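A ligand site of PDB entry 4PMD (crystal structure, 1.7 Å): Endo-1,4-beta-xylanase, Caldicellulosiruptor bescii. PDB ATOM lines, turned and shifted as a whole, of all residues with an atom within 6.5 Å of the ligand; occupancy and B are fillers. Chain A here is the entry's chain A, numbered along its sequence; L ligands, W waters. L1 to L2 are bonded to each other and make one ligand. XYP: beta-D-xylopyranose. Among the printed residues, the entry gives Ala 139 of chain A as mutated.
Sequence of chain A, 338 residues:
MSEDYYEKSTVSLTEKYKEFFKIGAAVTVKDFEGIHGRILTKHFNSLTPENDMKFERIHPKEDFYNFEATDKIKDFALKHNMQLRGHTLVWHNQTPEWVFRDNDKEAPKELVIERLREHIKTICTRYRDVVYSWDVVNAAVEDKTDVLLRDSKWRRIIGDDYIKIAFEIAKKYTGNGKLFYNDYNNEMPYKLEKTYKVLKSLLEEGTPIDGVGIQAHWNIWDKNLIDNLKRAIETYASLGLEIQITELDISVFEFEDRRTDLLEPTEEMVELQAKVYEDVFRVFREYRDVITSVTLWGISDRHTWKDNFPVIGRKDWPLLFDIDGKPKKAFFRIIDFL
O1 of XYP L1 lies within hydrogen-bond range of OE1 of Gln 215 (2.7 Å). The side-chain carboxylate (OE2) of Glu 50 lies within hydrogen-bond range of an oxygen (O2) of XYP L2 (2.7 Å). A ring nitrogen (NE2) of His 87 is in hydrogen-bond range of an oxygen (O3) of XYP L1, 2.7 Å away. OE2 of Glu 247 sits at hydrogen-bond distance from O2 of XYP L1, 2.7 Å away. NZ of Lys 54 sits at hydrogen-bond distance from O3 of XYP L1, 2.8 Å away. The indole nitrogen (NE1) of Trp 297 is in hydrogen-bond range of an oxygen (O2) of XYP L2 (2.9 Å). The side-chain amide nitrogen (ND2) of Asn 138 sits at hydrogen-bond distance from an oxygen (O2) of XYP L1, 3.0 Å away. The side-chain amide nitrogen (ND2) of Asn 51 sits at hydrogen-bond distance from an oxygen (O3) of XYP L2 (3.0 Å). The side-chain amide oxygen (OE1) of Gln 94 lies close to an oxygen (O5) of XYP L2.
The backbone carbonyl oxygen of Gln 215 sits close to the backbone NH of Glu 247, at 3.0 Å. ND2 of Asn 182 lies close to NE2 of Gln 215 (3.3 Å). O of Glu 50 sits at hydrogen-bond distance from NZ of Lys 54, at 3.1 Å. The side-chain carboxylate of Asp 135 sits at hydrogen-bond distance from a ring nitrogen (ND1) of His 87 (2.8 Å). A ring nitrogen (NE2) of His 217 lies within hydrogen-bond range of the side-chain carboxylate (OE1) of Glu 247 (2.7 Å). ND2 of Asn 182 is in hydrogen-bond range of OE2 of Glu 247 (3.1 Å). The side-chain amino group (NZ) of Lys 54 is in hydrogen-bond range of the side-chain amide oxygen (OE1) of Gln 94. The side-chain amide oxygen of Asn 51 lies within hydrogen-bond range of the side-chain amide nitrogen of Gln 94, at 3.1 Å.
Merely in contact with the ligand: Trp 91, Tyr 184, His 217 and Trp 305. Hydrophobic or aromatic side chains that line the ligand: His 87, Trp 91, Tyr 184, Trp 297 and Trp 305. 13 residues have an atom within 4 Å of the ligand: Glu 50, Asn 51, Lys 54, His 87, Trp 91, Gln 94, Asn 138, Tyr 184, Gln 215, His 217, Glu 247, Trp 297 and Trp 305.
Water W2 bridges NE1 of Trp 91 (2.9 Å) and O1 of XYP L1 (3.0 Å). Water W1 lies within hydrogen-bond range of OE2 of Glu 50 (2.7 Å) and O3 of XYP L2 (3.0 Å).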
ATOM      1  N   GLU A  50       3.805  26.175 -22.341  1.00  0.00           N
ATOM      2  CA  GLU A  50       3.755  26.137 -23.800  1.00  0.00           C
ATOM      3  C   GLU A  50       2.525  25.373 -24.256  1.00  0.00           C
ATOM      4  O   GLU A  50       1.920  25.709 -25.226  1.00  0.00           O
ATOM      5  CB  GLU A  50       5.030  25.469 -24.378  1.00  0.00           C
ATOM      6  CG  GLU A  50       5.109  25.543 -25.902  1.00  0.00           C
ATOM      7  CD  GLU A  50       6.254  24.751 -26.477  1.00  0.00           C
ATOM      8  OE1 GLU A  50       6.881  23.975 -25.715  1.00  0.00           O
ATOM      9  OE2 GLU A  50       6.482  24.865 -27.692  1.00  0.00           O
ATOM     10  N   ASN A  51       2.195  24.298 -23.536  1.00  0.00           N
ATOM     11  CA  ASN A  51       1.084  23.434 -23.897  1.00  0.00           C
ATOM     12  C   ASN A  51       0.208  22.996 -22.750  1.00  0.00           C
ATOM     13  O   ASN A  51      -0.940  22.618 -22.976  1.00  0.00           O
ATOM     14  CB  ASN A  51       1.588  22.183 -24.660  1.00  0.00           C
ATOM     15  CG  ASN A  51       1.997  22.525 -26.065  1.00  0.00           C
ATOM     16  OD1 ASN A  51       1.181  22.985 -26.884  1.00  0.00           O
ATOM     17  ND2 ASN A  51       3.286  22.342 -26.350  1.00  0.00           N
ATOM     18  N   LYS A  54      -3.375  24.278 -22.080  1.00  0.00           N
ATOM     19  CA  LYS A  54      -4.352  24.251 -23.182  1.00  0.00           C
ATOM     20  C   LYS A  54      -5.473  23.243 -22.889  1.00  0.00           C
ATOM     21  O   LYS A  54      -5.259  22.241 -22.194  1.00  0.00           O
ATOM     22  CB  LYS A  54      -3.688  23.952 -24.485  1.00  0.00           C
ATOM     23  CG  LYS A  54      -2.749  25.040 -24.899  1.00  0.00           C
ATOM     24  CD  LYS A  54      -1.885  24.658 -26.064  1.00  0.00           C
ATOM     25  CE  LYS A  54      -1.047  25.843 -26.501  1.00  0.00           C
ATOM     26  NZ  LYS A  54      -0.117  25.495 -27.567  1.00  0.00           N
ATOM     27  N   ARG A  57      -5.089  19.454 -23.150  1.00  0.00           N
ATOM     28  CA  ARG A  57      -4.078  18.891 -22.296  1.00  0.00           C
ATOM     29  C   ARG A  57      -4.524  18.849 -20.859  1.00  0.00           C
ATOM     30  O   ARG A  57      -4.422  17.805 -20.190  1.00  0.00           O
ATOM     31  CB  ARG A  57      -2.761  19.659 -22.386  1.00  0.00           C
ATOM     32  CG  ARG A  57      -2.145  19.721 -23.768  1.00  0.00           C
ATOM     33  CD  ARG A  57      -1.781  18.370 -24.323  1.00  0.00           C
ATOM     34  NE  ARG A  57      -1.209  18.521 -25.670  1.00  0.00           N
ATOM     35  CZ  ARG A  57       0.082  18.675 -25.947  1.00  0.00           C
ATOM     36  NH1 ARG A  57       0.464  18.824 -27.226  1.00  0.00           N
ATOM     37  NH2 ARG A  57       0.991  18.684 -24.969  1.00  0.00           N
ATOM     38  N   HIS A  87      -2.084  30.469 -20.404  1.00  0.00           N
ATOM     39  CA  HIS A  87      -2.275  30.258 -21.823  1.00  0.00           C
ATOM     40  C   HIS A  87      -2.841  28.882 -22.043  1.00  0.00           C
ATOM     41  O   HIS A  87      -2.146  27.896 -21.719  1.00  0.00           O
ATOM     42  CB  HIS A  87      -0.895  30.326 -22.513  1.00  0.00           C
ATOM     43  CG  HIS A  87      -0.924  30.174 -23.993  1.00  0.00           C
ATOM     44  ND1 HIS A  87      -1.405  31.161 -24.820  1.00  0.00           N
ATOM     45  CD2 HIS A  87      -0.581  29.137 -24.800  1.00  0.00           C
ATOM     46  CE1 HIS A  87      -1.345  30.747 -26.076  1.00  0.00           C
ATOM     47  NE2 HIS A  87      -0.871  29.523 -26.080  1.00  0.00           N
ATOM     48  N   THR A  88      -4.029  28.708 -22.583  1.00  0.00           N
ATOM     49  CA  THR A  88      -5.018  29.726 -22.976  1.00  0.00           C
ATOM     50  C   THR A  88      -6.405  29.073 -22.794  1.00  0.00           C
ATOM     51  O   THR A  88      -6.573  27.830 -22.807  1.00  0.00           O
ATOM     52  CB  THR A  88      -4.807  30.176 -24.450  1.00  0.00           C
ATOM     53  OG1 THR A  88      -5.860  31.076 -24.833  1.00  0.00           O
ATOM     54  CG2 THR A  88      -4.824  28.956 -25.387  1.00  0.00           C
ATOM     55  N   TRP A  91      -9.521  28.677 -27.461  1.00  0.00           N
ATOM     56  CA  TRP A  91      -8.769  28.678 -28.722  1.00  0.00           C
ATOM     57  C   TRP A  91      -9.403  27.652 -29.679  1.00  0.00           C
ATOM     58  O   TRP A  91      -9.876  26.610 -29.222  1.00  0.00           O
ATOM     59  CB  TRP A  91      -7.291  28.349 -28.455  1.00  0.00           C
ATOM     60  CG  TRP A  91      -6.324  28.450 -29.567  1.00  0.00           C
ATOM     61  CD1 TRP A  91      -6.354  29.292 -30.634  1.00  0.00           C
ATOM     62  CD2 TRP A  91      -5.078  27.738 -29.663  1.00  0.00           C
ATOM     63  NE1 TRP A  91      -5.240  29.124 -31.409  1.00  0.00           N
ATOM     64  CE2 TRP A  91      -4.456  28.149 -30.856  1.00  0.00           C
ATOM     65  CE3 TRP A  91      -4.497  26.716 -28.928  1.00  0.00           C
ATOM     66  CZ2 TRP A  91      -3.241  27.631 -31.278  1.00  0.00           C
ATOM     67  CZ3 TRP A  91      -3.293  26.218 -29.340  1.00  0.00           C
ATOM     68  CH2 TRP A  91      -2.670  26.669 -30.490  1.00  0.00           C
ATOM     69  N   GLN A  94      -6.188  22.821 -30.321  1.00  0.00           N
ATOM     70  CA  GLN A  94      -5.900  22.093 -29.080  1.00  0.00           C
ATOM     71  C   GLN A  94      -7.045  22.172 -28.063  1.00  0.00           C
ATOM     72  O   GLN A  94      -6.825  22.374 -26.849  1.00  0.00           O
ATOM     73  CB  GLN A  94      -4.543  22.513 -28.501  1.00  0.00           C
ATOM     74  CG  GLN A  94      -3.376  22.172 -29.434  1.00  0.00           C
ATOM     75  CD  GLN A  94      -2.024  22.593 -28.897  1.00  0.00           C
ATOM     76  OE1 GLN A  94      -1.469  23.597 -29.327  1.00  0.00           O
ATOM     77  NE2 GLN A  94      -1.472  21.807 -27.974  1.00  0.00           N
ATOM     78  N   ASP A 135      -4.383  34.593 -21.176  1.00  0.00           N
ATOM     79  CA  ASP A 135      -4.850  34.643 -22.577  1.00  0.00           C
ATOM     80  C   ASP A 135      -6.226  34.051 -22.590  1.00  0.00           C
ATOM     81  O   ASP A 135      -6.388  32.813 -22.694  1.00  0.00           O
ATOM     82  CB  ASP A 135      -3.925  33.869 -23.506  1.00  0.00           C
ATOM     83  CG  ASP A 135      -2.584  34.508 -23.646  1.00  0.00           C
ATOM     84  OD1 ASP A 135      -2.500  35.753 -23.571  1.00  0.00           O
ATOM     85  OD2 ASP A 135      -1.595  33.773 -23.876  1.00  0.00           O
ATOM     86  N   ASN A 138      -7.799  33.280 -27.668  1.00  0.00           N
ATOM     87  CA  ASN A 138      -6.613  33.219 -28.519  1.00  0.00           C
ATOM     88  C   ASN A 138      -7.022  33.077 -29.966  1.00  0.00           C
ATOM     89  O   ASN A 138      -7.794  32.210 -30.326  1.00  0.00           O
ATOM     90  CB  ASN A 138      -5.780  31.983 -28.089  1.00  0.00           C
ATOM     91  CG  ASN A 138      -4.318  32.083 -28.478  1.00  0.00           C
ATOM     92  OD1 ASN A 138      -3.687  33.125 -28.345  1.00  0.00           O
ATOM     93  ND2 ASN A 138      -3.762  30.990 -28.962  1.00  0.00           N
ATOM     94  N   ALA A 139      -6.526  33.993 -30.801  1.00  0.00           N
ATOM     95  CA  ALA A 139      -6.657  33.858 -32.282  1.00  0.00           C
ATOM     96  C   ALA A 139      -8.098  33.804 -32.809  1.00  0.00           C
ATOM     97  O   ALA A 139      -8.424  33.052 -33.697  1.00  0.00           O
ATOM     98  CB  ALA A 139      -5.822  32.658 -32.738  1.00  0.00           C
ATOM     99  N   ASN A 182      -5.239  37.481 -27.167  1.00  0.00           N
ATOM    100  CA  ASN A 182      -3.935  37.102 -27.744  1.00  0.00           C
ATOM    101  C   ASN A 182      -4.071  36.668 -29.199  1.00  0.00           C
ATOM    102  O   ASN A 182      -5.049  36.026 -29.546  1.00  0.00           O
ATOM    103  CB  ASN A 182      -3.314  35.969 -26.928  1.00  0.00           C
ATOM    104  CG  ASN A 182      -1.823  35.813 -27.161  1.00  0.00           C
ATOM    105  OD1 ASN A 182      -1.063  36.810 -27.269  1.00  0.00           O
ATOM    106  ND2 ASN A 182      -1.374  34.547 -27.244  1.00  0.00           N
ATOM    107  N   ASP A 183      -3.127  37.083 -30.047  1.00  0.00           N
ATOM    108  CA  ASP A 183      -3.186  36.765 -31.483  1.00  0.00           C
ATOM    109  C   ASP A 183      -1.843  36.979 -32.178  1.00  0.00           C
ATOM    110  O   ASP A 183      -0.957  37.639 -31.672  1.00  0.00           O
ATOM    111  CB  ASP A 183      -4.327  37.560 -32.157  1.00  0.00           C
ATOM    112  CG  ASP A 183      -4.993  36.828 -33.291  1.00  0.00           C
ATOM    113  OD1 ASP A 183      -4.435  35.838 -33.835  1.00  0.00           O
ATOM    114  OD2 ASP A 183      -6.149  37.210 -33.630  1.00  0.00           O
ATOM    115  N   TYR A 184      -1.726  36.372 -33.370  1.00  0.00           N
ATOM    116  CA  TYR A 184      -0.539  36.477 -34.232  1.00  0.00           C
ATOM    117  C   TYR A 184      -0.903  37.349 -35.441  1.00  0.00           C
ATOM    118  O   TYR A 184      -2.072  37.529 -35.787  1.00  0.00           O
ATOM    119  CB  TYR A 184      -0.058  35.087 -34.697  1.00  0.00           C
ATOM    120  CG  TYR A 184      -1.054  34.344 -35.515  1.00  0.00           C
ATOM    121  CD1 TYR A 184      -2.039  33.559 -34.925  1.00  0.00           C
ATOM    122  CD2 TYR A 184      -1.043  34.427 -36.907  1.00  0.00           C
ATOM    123  CE1 TYR A 184      -2.967  32.869 -35.660  1.00  0.00           C
ATOM    124  CE2 TYR A 184      -1.986  33.748 -37.673  1.00  0.00           C
ATOM    125  CZ  TYR A 184      -2.950  32.962 -37.058  1.00  0.00           C
ATOM    126  OH  TYR A 184      -3.825  32.297 -37.840  1.00  0.00           O
ATOM    127  N   GLN A 215       1.598  38.158 -30.339  1.00  0.00           N
ATOM    128  CA  GLN A 215       2.386  36.929 -30.267  1.00  0.00           C
ATOM    129  C   GLN A 215       3.822  37.090 -30.751  1.00  0.00           C
ATOM    130  O   GLN A 215       4.721  36.572 -30.186  1.00  0.00           O
ATOM    131  CB  GLN A 215       1.705  35.790 -30.980  1.00  0.00           C
ATOM    132  CG  GLN A 215       0.514  35.206 -30.218  1.00  0.00           C
ATOM    133  CD  GLN A 215      -0.149  34.064 -30.915  1.00  0.00           C
ATOM    134  OE1 GLN A 215       0.397  33.517 -31.880  1.00  0.00           O
ATOM    135  NE2 GLN A 215      -1.345  33.723 -30.478  1.00  0.00           N
ATOM    136  N   HIS A 217       5.346  36.085 -33.612  1.00  0.00           N
ATOM    137  CA  HIS A 217       6.001  35.019 -34.356  1.00  0.00           C
ATOM    138  C   HIS A 217       6.502  35.620 -35.667  1.00  0.00           C
ATOM    139  O   HIS A 217       5.824  35.627 -36.687  1.00  0.00           O
ATOM    140  CB  HIS A 217       5.031  33.861 -34.569  1.00  0.00           C
ATOM    141  CG  HIS A 217       4.745  33.105 -33.304  1.00  0.00           C
ATOM    142  ND1 HIS A 217       5.722  32.466 -32.592  1.00  0.00           N
ATOM    143  CD2 HIS A 217       3.595  32.928 -32.599  1.00  0.00           C
ATOM    144  CE1 HIS A 217       5.192  31.924 -31.495  1.00  0.00           C
ATOM    145  NE2 HIS A 217       3.907  32.169 -31.501  1.00  0.00           N
ATOM    146  N   GLU A 247       4.767  35.705 -27.335  1.00  0.00           N
ATOM    147  CA  GLU A 247       5.321  34.480 -27.904  1.00  0.00           C
ATOM    148  C   GLU A 247       6.438  34.787 -28.883  1.00  0.00           C
ATOM    149  O   GLU A 247       6.563  34.144 -29.936  1.00  0.00           O
ATOM    150  CB  GLU A 247       4.232  33.658 -28.579  1.00  0.00           C
ATOM    151  CG  GLU A 247       2.999  33.414 -27.729  1.00  0.00           C
ATOM    152  CD  GLU A 247       1.970  32.520 -28.363  1.00  0.00           C
ATOM    153  OE1 GLU A 247       2.208  31.864 -29.409  1.00  0.00           O
ATOM    154  OE2 GLU A 247       0.872  32.424 -27.742  1.00  0.00           O
ATOM    155  N   TRP A 297       9.049  32.566 -27.023  1.00  0.00           N
ATOM    156  CA  TRP A 297       8.392  31.271 -27.135  1.00  0.00           C
ATOM    157  C   TRP A 297       9.418  30.137 -27.084  1.00  0.00           C
ATOM    158  O   TRP A 297       9.489  29.314 -27.962  1.00  0.00           O
ATOM    159  CB  TRP A 297       7.523  31.205 -28.363  1.00  0.00           C
ATOM    160  CG  TRP A 297       6.340  30.245 -28.182  1.00  0.00           C
ATOM    161  CD1 TRP A 297       6.060  29.136 -28.913  1.00  0.00           C
ATOM    162  CD2 TRP A 297       5.316  30.329 -27.187  1.00  0.00           C
ATOM    163  NE1 TRP A 297       4.915  28.516 -28.464  1.00  0.00           N
ATOM    164  CE2 TRP A 297       4.439  29.225 -27.392  1.00  0.00           C
ATOM    165  CE3 TRP A 297       5.045  31.226 -26.150  1.00  0.00           C
ATOM    166  CZ2 TRP A 297       3.306  28.998 -26.582  1.00  0.00           C
ATOM    167  CZ3 TRP A 297       3.921  30.983 -25.328  1.00  0.00           C
ATOM    168  CH2 TRP A 297       3.087  29.896 -25.553  1.00  0.00           C
ATOM    169  N   THR A 304      12.450  24.259 -29.723  1.00  0.00           N
ATOM    170  CA  THR A 304      11.591  25.290 -30.330  1.00  0.00           C
ATOM    171  C   THR A 304      10.543  24.616 -31.223  1.00  0.00           C
ATOM    172  O   THR A 304      10.829  23.677 -31.992  1.00  0.00           O
ATOM    173  CB  THR A 304      12.366  26.373 -31.132  1.00  0.00           C
ATOM    174  OG1 THR A 304      11.435  27.173 -31.881  1.00  0.00           O
ATOM    175  CG2 THR A 304      13.367  25.767 -32.100  1.00  0.00           C
ATOM    176  N   TRP A 305       9.314  25.114 -31.120  1.00  0.00           N
ATOM    177  CA  TRP A 305       8.237  24.609 -31.961  1.00  0.00           C
ATOM    178  C   TRP A 305       8.537  24.878 -33.450  1.00  0.00           C
ATOM    179  O   TRP A 305       7.913  24.296 -34.333  1.00  0.00           O
ATOM    180  CB  TRP A 305       6.905  25.257 -31.587  1.00  0.00           C
ATOM    181  CG  TRP A 305       6.676  26.648 -32.075  1.00  0.00           C
ATOM    182  CD1 TRP A 305       7.448  27.742 -31.841  1.00  0.00           C
ATOM    183  CD2 TRP A 305       5.576  27.095 -32.878  1.00  0.00           C
ATOM    184  NE1 TRP A 305       6.890  28.838 -32.429  1.00  0.00           N
ATOM    185  CE2 TRP A 305       5.746  28.478 -33.077  1.00  0.00           C
ATOM    186  CE3 TRP A 305       4.473  26.455 -33.455  1.00  0.00           C
ATOM    187  CZ2 TRP A 305       4.864  29.220 -33.861  1.00  0.00           C
ATOM    188  CZ3 TRP A 305       3.602  27.211 -34.235  1.00  0.00           C
ATOM    189  CH2 TRP A 305       3.785  28.570 -34.411  1.00  0.00           C
HETATM  190  O1  XYP L   1      -0.655  31.098 -32.142  1.00  0.00           O
HETATM  191  C1  XYP L   1       0.316  30.420 -31.352  1.00  0.00           C
HETATM  192  C2  XYP L   1      -0.381  29.831 -30.118  1.00  0.00           C
HETATM  193  C3  XYP L   1       0.510  28.870 -29.345  1.00  0.00           C
HETATM  194  C4  XYP L   1       1.159  27.886 -30.317  1.00  0.00           C
HETATM  195  C5  XYP L   1       1.886  28.667 -31.395  1.00  0.00           C
HETATM  196  O2  XYP L   1      -0.813  30.877 -29.261  1.00  0.00           O
HETATM  197  O3  XYP L   1      -0.180  28.175 -28.304  1.00  0.00           O
HETATM  198  O4  XYP L   1       2.051  27.084 -29.587  1.00  0.00           O
HETATM  199  O5  XYP L   1       0.942  29.417 -32.115  1.00  0.00           O
HETATM  200  C1  XYP L   2       2.287  25.856 -30.217  1.00  0.00           C
HETATM  201  C2  XYP L   2       3.305  25.078 -29.406  1.00  0.00           C
HETATM  202  C3  XYP L   2       3.513  23.667 -29.966  1.00  0.00           C
HETATM  203  C4  XYP L   2       2.187  22.986 -30.246  1.00  0.00           C
HETATM  204  C5  XYP L   2       1.237  23.896 -30.996  1.00  0.00           C
HETATM  205  O2  XYP L   2       4.518  25.779 -29.266  1.00  0.00           O
HETATM  206  O3  XYP L   2       4.316  22.891 -29.091  1.00  0.00           O
HETATM  207  O4  XYP L   2       2.413  21.779 -30.977  1.00  0.00           O
HETATM  208  O5  XYP L   2       1.096  25.108 -30.297  1.00  0.00           O
HETATM  209  O   HOH W   1       7.345  22.761 -29.195  1.00  0.00           O
HETATM  210  O   HOH W   2      -3.332  30.328 -33.256  1.00  0.00           O
